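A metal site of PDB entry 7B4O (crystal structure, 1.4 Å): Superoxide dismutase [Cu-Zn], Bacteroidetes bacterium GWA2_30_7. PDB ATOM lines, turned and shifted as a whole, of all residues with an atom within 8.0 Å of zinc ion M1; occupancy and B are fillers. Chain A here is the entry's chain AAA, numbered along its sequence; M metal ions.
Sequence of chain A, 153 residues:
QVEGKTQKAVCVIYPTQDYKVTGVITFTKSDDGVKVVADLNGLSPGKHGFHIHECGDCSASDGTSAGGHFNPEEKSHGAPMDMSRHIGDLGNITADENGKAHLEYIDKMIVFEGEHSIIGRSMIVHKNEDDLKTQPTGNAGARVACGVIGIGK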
ATOM      1  N   GLY A  49     -16.680 -12.348   8.100  1.00  0.00           N
ATOM      2  CA  GLY A  49     -15.700 -11.606   8.895  1.00  0.00           C
ATOM      3  C   GLY A  49     -15.038 -10.512   8.084  1.00  0.00           C
ATOM      4  O   GLY A  49     -14.661 -10.742   6.930  1.00  0.00           O
ATOM      5  N   PHE A  50     -14.881  -9.361   8.708  1.00  0.00           N
ATOM      6  CA  PHE A  50     -14.468  -8.105   8.042  1.00  0.00           C
ATOM      7  C   PHE A  50     -13.476  -7.422   8.984  1.00  0.00           C
ATOM      8  O   PHE A  50     -13.903  -6.846  10.001  1.00  0.00           O
ATOM      9  CB  PHE A  50     -15.720  -7.259   7.774  1.00  0.00           C
ATOM     10  CG  PHE A  50     -15.507  -5.995   6.993  1.00  0.00           C
ATOM     11  CD1 PHE A  50     -15.297  -6.017   5.623  1.00  0.00           C
ATOM     12  CD2 PHE A  50     -15.581  -4.768   7.635  1.00  0.00           C
ATOM     13  CE1 PHE A  50     -15.121  -4.834   4.917  1.00  0.00           C
ATOM     14  CE2 PHE A  50     -15.415  -3.583   6.929  1.00  0.00           C
ATOM     15  CZ  PHE A  50     -15.185  -3.616   5.570  1.00  0.00           C
ATOM     16  N   HIS A  51     -12.175  -7.537   8.705  1.00  0.00           N
ATOM     17  CA  HIS A  51     -11.129  -7.194   9.688  1.00  0.00           C
ATOM     18  C   HIS A  51      -9.998  -6.382   9.078  1.00  0.00           C
ATOM     19  O   HIS A  51      -9.657  -6.572   7.898  1.00  0.00           O
ATOM     20  CB  HIS A  51     -10.494  -8.452  10.273  1.00  0.00           C
ATOM     21  CG  HIS A  51     -11.451  -9.398  10.896  1.00  0.00           C
ATOM     22  ND1 HIS A  51     -11.246 -10.757  10.797  1.00  0.00           N
ATOM     23  CD2 HIS A  51     -12.587  -9.201  11.592  1.00  0.00           C
ATOM     24  CE1 HIS A  51     -12.212 -11.371  11.457  1.00  0.00           C
ATOM     25  NE2 HIS A  51     -13.061 -10.436  11.930  1.00  0.00           N
ATOM     26  N   ILE A  52      -9.396  -5.547   9.924  1.00  0.00           N
ATOM     27  CA  ILE A  52      -8.073  -4.956   9.612  1.00  0.00           C
ATOM     28  C   ILE A  52      -7.029  -5.910  10.175  1.00  0.00           C
ATOM     29  O   ILE A  52      -7.073  -6.209  11.426  1.00  0.00           O
ATOM     30  CB  ILE A  52      -7.910  -3.539  10.185  1.00  0.00           C
ATOM     31  CG1 ILE A  52      -9.081  -2.638   9.803  1.00  0.00           C
ATOM     32  CG2 ILE A  52      -6.577  -2.964   9.773  1.00  0.00           C
ATOM     33  CD1 ILE A  52      -8.984  -1.240  10.345  1.00  0.00           C
ATOM     34  N   HIS A  53      -6.141  -6.402   9.326  1.00  0.00           N
ATOM     35  CA  HIS A  53      -5.025  -7.278   9.739  1.00  0.00           C
ATOM     36  C   HIS A  53      -3.742  -6.455   9.801  1.00  0.00           C
ATOM     37  O   HIS A  53      -3.703  -5.332   9.279  1.00  0.00           O
ATOM     38  CB  HIS A  53      -4.961  -8.514   8.842  1.00  0.00           C
ATOM     39  CG  HIS A  53      -5.987  -9.559   9.155  1.00  0.00           C
ATOM     40  ND1 HIS A  53      -5.637 -10.863   9.399  1.00  0.00           N
ATOM     41  CD2 HIS A  53      -7.322  -9.516   9.248  1.00  0.00           C
ATOM     42  CE1 HIS A  53      -6.720 -11.585   9.642  1.00  0.00           C
ATOM     43  NE2 HIS A  53      -7.779 -10.802   9.513  1.00  0.00           N
ATOM     44  N   GLY A  67      -0.973 -11.472   8.024  1.00  0.00           N
ATOM     45  CA  GLY A  67      -0.754 -11.730   9.454  1.00  0.00           C
ATOM     46  C   GLY A  67      -2.059 -11.752  10.230  1.00  0.00           C
ATOM     47  O   GLY A  67      -3.116 -12.019   9.632  1.00  0.00           O
ATOM     48  N   GLY A  68      -1.993 -11.542  11.537  1.00  0.00           N
ATOM     49  CA  GLY A  68      -3.143 -11.614  12.442  1.00  0.00           C
ATOM     50  C   GLY A  68      -3.896 -10.305  12.508  1.00  0.00           C
ATOM     51  O   GLY A  68      -3.630  -9.411  11.684  1.00  0.00           O
ATOM     52  N   HIS A  69      -4.823 -10.190  13.449  1.00  0.00           N
ATOM     53  CA  HIS A  69      -5.654  -8.975  13.597  1.00  0.00           C
ATOM     54  C   HIS A  69      -4.770  -7.800  13.993  1.00  0.00           C
ATOM     55  O   HIS A  69      -3.816  -7.978  14.788  1.00  0.00           O
ATOM     56  CB  HIS A  69      -6.813  -9.205  14.571  1.00  0.00           C
ATOM     57  CG  HIS A  69      -7.816 -10.131  13.986  1.00  0.00           C
ATOM     58  ND1 HIS A  69      -9.055 -10.351  14.543  1.00  0.00           N
ATOM     59  CD2 HIS A  69      -7.784 -10.837  12.825  1.00  0.00           C
ATOM     60  CE1 HIS A  69      -9.741 -11.169  13.764  1.00  0.00           C
ATOM     61  NE2 HIS A  69      -8.976 -11.499  12.705  1.00  0.00           N
ATOM     62  N   PHE A  70      -5.070  -6.626  13.453  1.00  0.00           N
ATOM     63  CA  PHE A  70      -4.378  -5.396  13.888  1.00  0.00           C
ATOM     64  C   PHE A  70      -4.778  -5.129  15.345  1.00  0.00           C
ATOM     65  O   PHE A  70      -5.962  -4.858  15.648  1.00  0.00           O
ATOM     66  CB  PHE A  70      -4.699  -4.235  12.951  1.00  0.00           C
ATOM     67  CG  PHE A  70      -4.015  -2.958  13.313  1.00  0.00           C
ATOM     68  CD1 PHE A  70      -2.655  -2.932  13.553  1.00  0.00           C
ATOM     69  CD2 PHE A  70      -4.723  -1.773  13.404  1.00  0.00           C
ATOM     70  CE1 PHE A  70      -2.009  -1.746  13.868  1.00  0.00           C
ATOM     71  CE2 PHE A  70      -4.074  -0.582  13.739  1.00  0.00           C
ATOM     72  CZ  PHE A  70      -2.729  -0.579  13.964  1.00  0.00           C
ATOM     73  N   HIS A  77     -10.080 -10.388  21.093  1.00  0.00           N
ATOM     74  CA  HIS A  77     -10.961 -10.282  19.915  1.00  0.00           C
ATOM     75  C   HIS A  77     -12.395  -9.998  20.386  1.00  0.00           C
ATOM     76  O   HIS A  77     -12.837 -10.648  21.349  1.00  0.00           O
ATOM     77  CB  HIS A  77     -10.918 -11.550  19.090  1.00  0.00           C
ATOM     78  CG  HIS A  77     -11.777 -11.477  17.875  1.00  0.00           C
ATOM     79  ND1 HIS A  77     -11.459 -10.702  16.763  1.00  0.00           N
ATOM     80  CD2 HIS A  77     -12.998 -11.999  17.633  1.00  0.00           C
ATOM     81  CE1 HIS A  77     -12.431 -10.810  15.892  1.00  0.00           C
ATOM     82  NE2 HIS A  77     -13.385 -11.601  16.385  1.00  0.00           N
ATOM     83  N   HIS A  86      -9.961  -5.862  19.297  1.00  0.00           N
ATOM     84  CA  HIS A  86      -8.799  -5.424  18.491  1.00  0.00           C
ATOM     85  C   HIS A  86      -9.203  -4.166  17.737  1.00  0.00           C
ATOM     86  O   HIS A  86     -10.386  -4.036  17.381  1.00  0.00           O
ATOM     87  CB  HIS A  86      -8.419  -6.531  17.489  1.00  0.00           C
ATOM     88  CG  HIS A  86      -8.071  -7.835  18.116  1.00  0.00           C
ATOM     89  ND1 HIS A  86      -8.375  -9.037  17.540  1.00  0.00           N
ATOM     90  CD2 HIS A  86      -7.449  -8.108  19.278  1.00  0.00           C
ATOM     91  CE1 HIS A  86      -7.914  -9.998  18.312  1.00  0.00           C
ATOM     92  NE2 HIS A  86      -7.351  -9.467  19.377  1.00  0.00           N
ATOM     93  N   GLY A  88      -8.600  -3.781  14.816  1.00  0.00           N
ATOM     94  CA  GLY A  88      -9.022  -4.330  13.503  1.00  0.00           C
ATOM     95  C   GLY A  88     -10.363  -5.034  13.512  1.00  0.00           C
ATOM     96  O   GLY A  88     -10.735  -5.579  12.450  1.00  0.00           O
ATOM     97  N   ASP A  89     -11.092  -5.099  14.628  1.00  0.00           N
ATOM     98  CA  ASP A  89     -12.346  -5.875  14.727  1.00  0.00           C
ATOM     99  C   ASP A  89     -13.532  -5.072  14.194  1.00  0.00           C
ATOM    100  O   ASP A  89     -14.217  -4.414  14.982  1.00  0.00           O
ATOM    101  CB  ASP A  89     -12.578  -6.365  16.156  1.00  0.00           C
ATOM    102  CG  ASP A  89     -11.585  -7.445  16.557  1.00  0.00           C
ATOM    103  OD1 ASP A  89     -10.892  -7.996  15.661  1.00  0.00           O
ATOM    104  OD2 ASP A  89     -11.505  -7.716  17.778  1.00  0.00           O
ATOM    105  N   GLY A  91     -16.111  -6.434  12.642  1.00  0.00           N
ATOM    106  CA  GLY A  91     -17.308  -7.287  12.712  1.00  0.00           C
ATOM    107  C   GLY A  91     -17.522  -8.093  11.435  1.00  0.00           C
ATOM    108  O   GLY A  91     -16.582  -8.773  10.986  1.00  0.00           O
ATOM    109  N   MET A 123      -7.022  -4.870   4.834  1.00  0.00           N
ATOM    110  CA  MET A 123      -8.382  -5.388   5.039  1.00  0.00           C
ATOM    111  C   MET A 123      -8.370  -6.850   4.592  1.00  0.00           C
ATOM    112  O   MET A 123      -7.815  -7.148   3.508  1.00  0.00           O
ATOM    113  CB  MET A 123      -9.427  -4.595   4.245  1.00  0.00           C
ATOM    114  CG  MET A 123      -9.716  -3.206   4.800  1.00  0.00           C
ATOM    115  SD  MET A 123     -10.371  -3.265   6.485  1.00  0.00           S
ATOM    116  CE  MET A 123     -11.733  -4.411   6.290  1.00  0.00           C
ATOM    117  N   ILE A 124      -8.946  -7.714   5.413  1.00  0.00           N
ATOM    118  CA  ILE A 124      -9.194  -9.137   5.068  1.00  0.00           C
ATOM    119  C   ILE A 124     -10.690  -9.367   5.190  1.00  0.00           C
ATOM    120  O   ILE A 124     -11.283  -9.010   6.194  1.00  0.00           O
ATOM    121  CB  ILE A 124      -8.388 -10.081   5.964  1.00  0.00           C
ATOM    122  CG1 ILE A 124      -6.880  -9.977   5.715  1.00  0.00           C
ATOM    123  CG2 ILE A 124      -8.868 -11.514   5.791  1.00  0.00           C
ATOM    124  CD1 ILE A 124      -6.440 -10.498   4.343  1.00  0.00           C
ATOM    125  N   VAL A 125     -11.262  -9.972   4.154  1.00  0.00           N
ATOM    126  CA  VAL A 125     -12.654 -10.492   4.209  1.00  0.00           C
ATOM    127  C   VAL A 125     -12.537 -12.006   4.321  1.00  0.00           C
ATOM    128  O   VAL A 125     -11.715 -12.615   3.640  1.00  0.00           O
ATOM    129  CB  VAL A 125     -13.485 -10.036   3.006  1.00  0.00           C
ATOM    130  CG1 VAL A 125     -14.913 -10.551   3.104  1.00  0.00           C
ATOM    131  CG2 VAL A 125     -13.453  -8.529   2.859  1.00  0.00           C
ATOM    132  N   HIS A 126     -13.329 -12.586   5.212  1.00  0.00           N
ATOM    133  CA  HIS A 126     -13.288 -14.028   5.532  1.00  0.00           C
ATOM    134  C   HIS A 126     -14.425 -14.792   4.862  1.00  0.00           C
ATOM    135  O   HIS A 126     -15.440 -14.211   4.486  1.00  0.00           O
ATOM    136  CB  HIS A 126     -13.288 -14.227   7.044  1.00  0.00           C
ATOM    137  CG  HIS A 126     -12.014 -13.835   7.713  1.00  0.00           C
ATOM    138  ND1 HIS A 126     -10.952 -14.709   7.811  1.00  0.00           N
ATOM    139  CD2 HIS A 126     -11.635 -12.693   8.336  1.00  0.00           C
ATOM    140  CE1 HIS A 126      -9.962 -14.100   8.450  1.00  0.00           C
ATOM    141  NE2 HIS A 126     -10.350 -12.871   8.806  1.00  0.00           N
ATOM    142  N   ASP A 130     -17.627 -13.966  11.478  1.00  0.00           N
ATOM    143  CA  ASP A 130     -16.890 -13.722  12.736  1.00  0.00           C
ATOM    144  C   ASP A 130     -17.896 -13.890  13.875  1.00  0.00           C
ATOM    145  O   ASP A 130     -18.874 -13.123  13.895  1.00  0.00           O
ATOM    146  CB  ASP A 130     -16.278 -12.320  12.685  1.00  0.00           C
ATOM    147  CG  ASP A 130     -15.523 -11.875  13.924  1.00  0.00           C
ATOM    148  OD1 ASP A 130     -15.633 -12.523  14.985  1.00  0.00           O
ATOM    149  OD2 ASP A 130     -14.839 -10.846  13.828  1.00  0.00           O
ATOM    150  N   PRO A 136      -8.332 -16.335  19.044  1.00  0.00           N
ATOM    151  CA  PRO A 136      -8.163 -14.886  18.947  1.00  0.00           C
ATOM    152  C   PRO A 136      -8.720 -14.190  17.679  1.00  0.00           C
ATOM    153  O   PRO A 136      -8.465 -13.011  17.502  1.00  0.00           O
ATOM    154  CB  PRO A 136      -6.629 -14.784  18.912  1.00  0.00           C
ATOM    155  CG  PRO A 136      -6.211 -15.988  18.083  1.00  0.00           C
ATOM    156  CD  PRO A 136      -7.230 -17.061  18.412  1.00  0.00           C
ATOM    157  N   THR A 137      -9.467 -14.911  16.843  1.00  0.00           N
ATOM    158  CA  THR A 137      -9.868 -14.422  15.493  1.00  0.00           C
ATOM    159  C   THR A 137     -11.380 -14.442  15.238  1.00  0.00           C
ATOM    160  O   THR A 137     -11.742 -13.963  14.165  1.00  0.00           O
ATOM    161  CB  THR A 137      -9.167 -15.223  14.385  1.00  0.00           C
ATOM    162  OG1 THR A 137      -9.811 -16.495  14.275  1.00  0.00           O
ATOM    163  CG2 THR A 137      -7.700 -15.444  14.650  1.00  0.00           C
ATOM    164  N   GLY A 138     -12.225 -14.972  16.134  1.00  0.00           N
ATOM    165  CA  GLY A 138     -13.682 -15.088  15.854  1.00  0.00           C
ATOM    166  C   GLY A 138     -14.044 -16.243  14.933  1.00  0.00           C
ATOM    167  O   GLY A 138     -15.222 -16.332  14.534  1.00  0.00           O
ATOM    168  N   ASN A 139     -13.082 -17.112  14.618  1.00  0.00           N
ATOM    169  CA  ASN A 139     -13.305 -18.377  13.873  1.00  0.00           C
ATOM    170  C   ASN A 139     -13.982 -18.103  12.519  1.00  0.00           C
ATOM    171  O   ASN A 139     -14.877 -18.872  12.124  1.00  0.00           O
ATOM    172  CB  ASN A 139     -14.156 -19.333  14.723  1.00  0.00           C
ATOM    173  CG  ASN A 139     -14.155 -20.760  14.198  1.00  0.00           C
ATOM    174  OD1 ASN A 139     -13.150 -21.240  13.674  1.00  0.00           O
ATOM    175  ND2 ASN A 139     -15.280 -21.439  14.343  1.00  0.00           N
ATOM    176  N   ALA A 140     -13.519 -17.094  11.802  1.00  0.00           N
ATOM    177  CA  ALA A 140     -14.125 -16.654  10.526  1.00  0.00           C
ATOM    178  C   ALA A 140     -13.562 -17.464   9.353  1.00  0.00           C
ATOM    179  O   ALA A 140     -14.007 -17.239   8.213  1.00  0.00           O
ATOM    180  CB  ALA A 140     -13.927 -15.170  10.336  1.00  0.00           C
ATOM    181  N   GLY A 141     -12.614 -18.360   9.592  1.00  0.00           N
ATOM    182  CA  GLY A 141     -12.117 -19.273   8.553  1.00  0.00           C
ATOM    183  C   GLY A 141     -11.266 -18.562   7.511  1.00  0.00           C
ATOM    184  O   GLY A 141     -10.576 -17.573   7.847  1.00  0.00           O
ATOM    185  N   ALA A 142     -11.300 -19.068   6.280  1.00  0.00           N
ATOM    186  CA  ALA A 142     -10.332 -18.718   5.227  1.00  0.00           C
ATOM    187  C   ALA A 142     -10.464 -17.239   4.836  1.00  0.00           C
ATOM    188  O   ALA A 142     -11.511 -16.586   5.118  1.00  0.00           O
ATOM    189  CB  ALA A 142     -10.523 -19.618   4.043  1.00  0.00           C
ATOM    190  N   ARG A 143      -9.421 -16.733   4.203  1.00  0.00           N
ATOM    191  CA  ARG A 143      -9.348 -15.334   3.726  1.00  0.00           C
ATOM    192  C   ARG A 143      -9.742 -15.344   2.253  1.00  0.00           C
ATOM    193  O   ARG A 143      -9.063 -16.043   1.465  1.00  0.00           O
ATOM    194  CB  ARG A 143      -7.937 -14.821   3.950  1.00  0.00           C
ATOM    195  CG  ARG A 143      -7.486 -14.952   5.387  1.00  0.00           C
ATOM    196  CD  ARG A 143      -6.041 -14.561   5.635  1.00  0.00           C
ATOM    197  NE  ARG A 143      -5.759 -14.792   7.042  1.00  0.00           N
ATOM    198  CZ  ARG A 143      -4.842 -14.165   7.757  1.00  0.00           C
ATOM    199  NH1 ARG A 143      -4.046 -13.259   7.223  1.00  0.00           N
ATOM    200  NH2 ARG A 143      -4.711 -14.458   9.039  1.00  0.00           N
HETATM  201 ZN    ZN M   1      -9.501 -11.697  10.104  1.00  0.00          ZN
HETATM  202 ZN    ZN M   2      -9.856  -9.501  16.259  1.00  0.00          ZN
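NE2 of His 51 lies within hydrogen-bond range of OD2 of Asp 130 (2.6 Å).
The backbone carbonyl oxygen of Gly 67 lies within hydrogen-bond range of a ring nitrogen (ND1) of His 53 (2.8 Å).
O of His 51 is in hydrogen-bond range of N of Ile 124 (2.8 Å).
The backbone carbonyl oxygen (O) of Gly 141 sits at hydrogen-bond distance from a ring nitrogen (ND1) of His 126 (2.9 Å).
A ring nitrogen (NE2) of His 53 sits close to a ring nitrogen (NE2) of His 69 (3.5 Å).
ND1 of His 126 sits close to O of Ala 142 (3.3 Å).
ND1 of His 53 lies close to O of Gly 68, 3.4 Å away.
The backbone NH of His 126 is in hydrogen-bond range of the backbone carbonyl oxygen of Gly 49 (2.9 Å).
Zinc ion M1 is bound by a ring nitrogen (NE2) of His 126.
Zinc ion M1 is bound by NE2 of His 53 (2.0 Å).
Zinc ion M1 is bound by ND1 of His 51 (2.1 Å).
Zinc ion M1 has three donor atoms within binding distance.
Slightly farther from zinc ion M1 lies NE2 of His 69 (2.7 Å).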
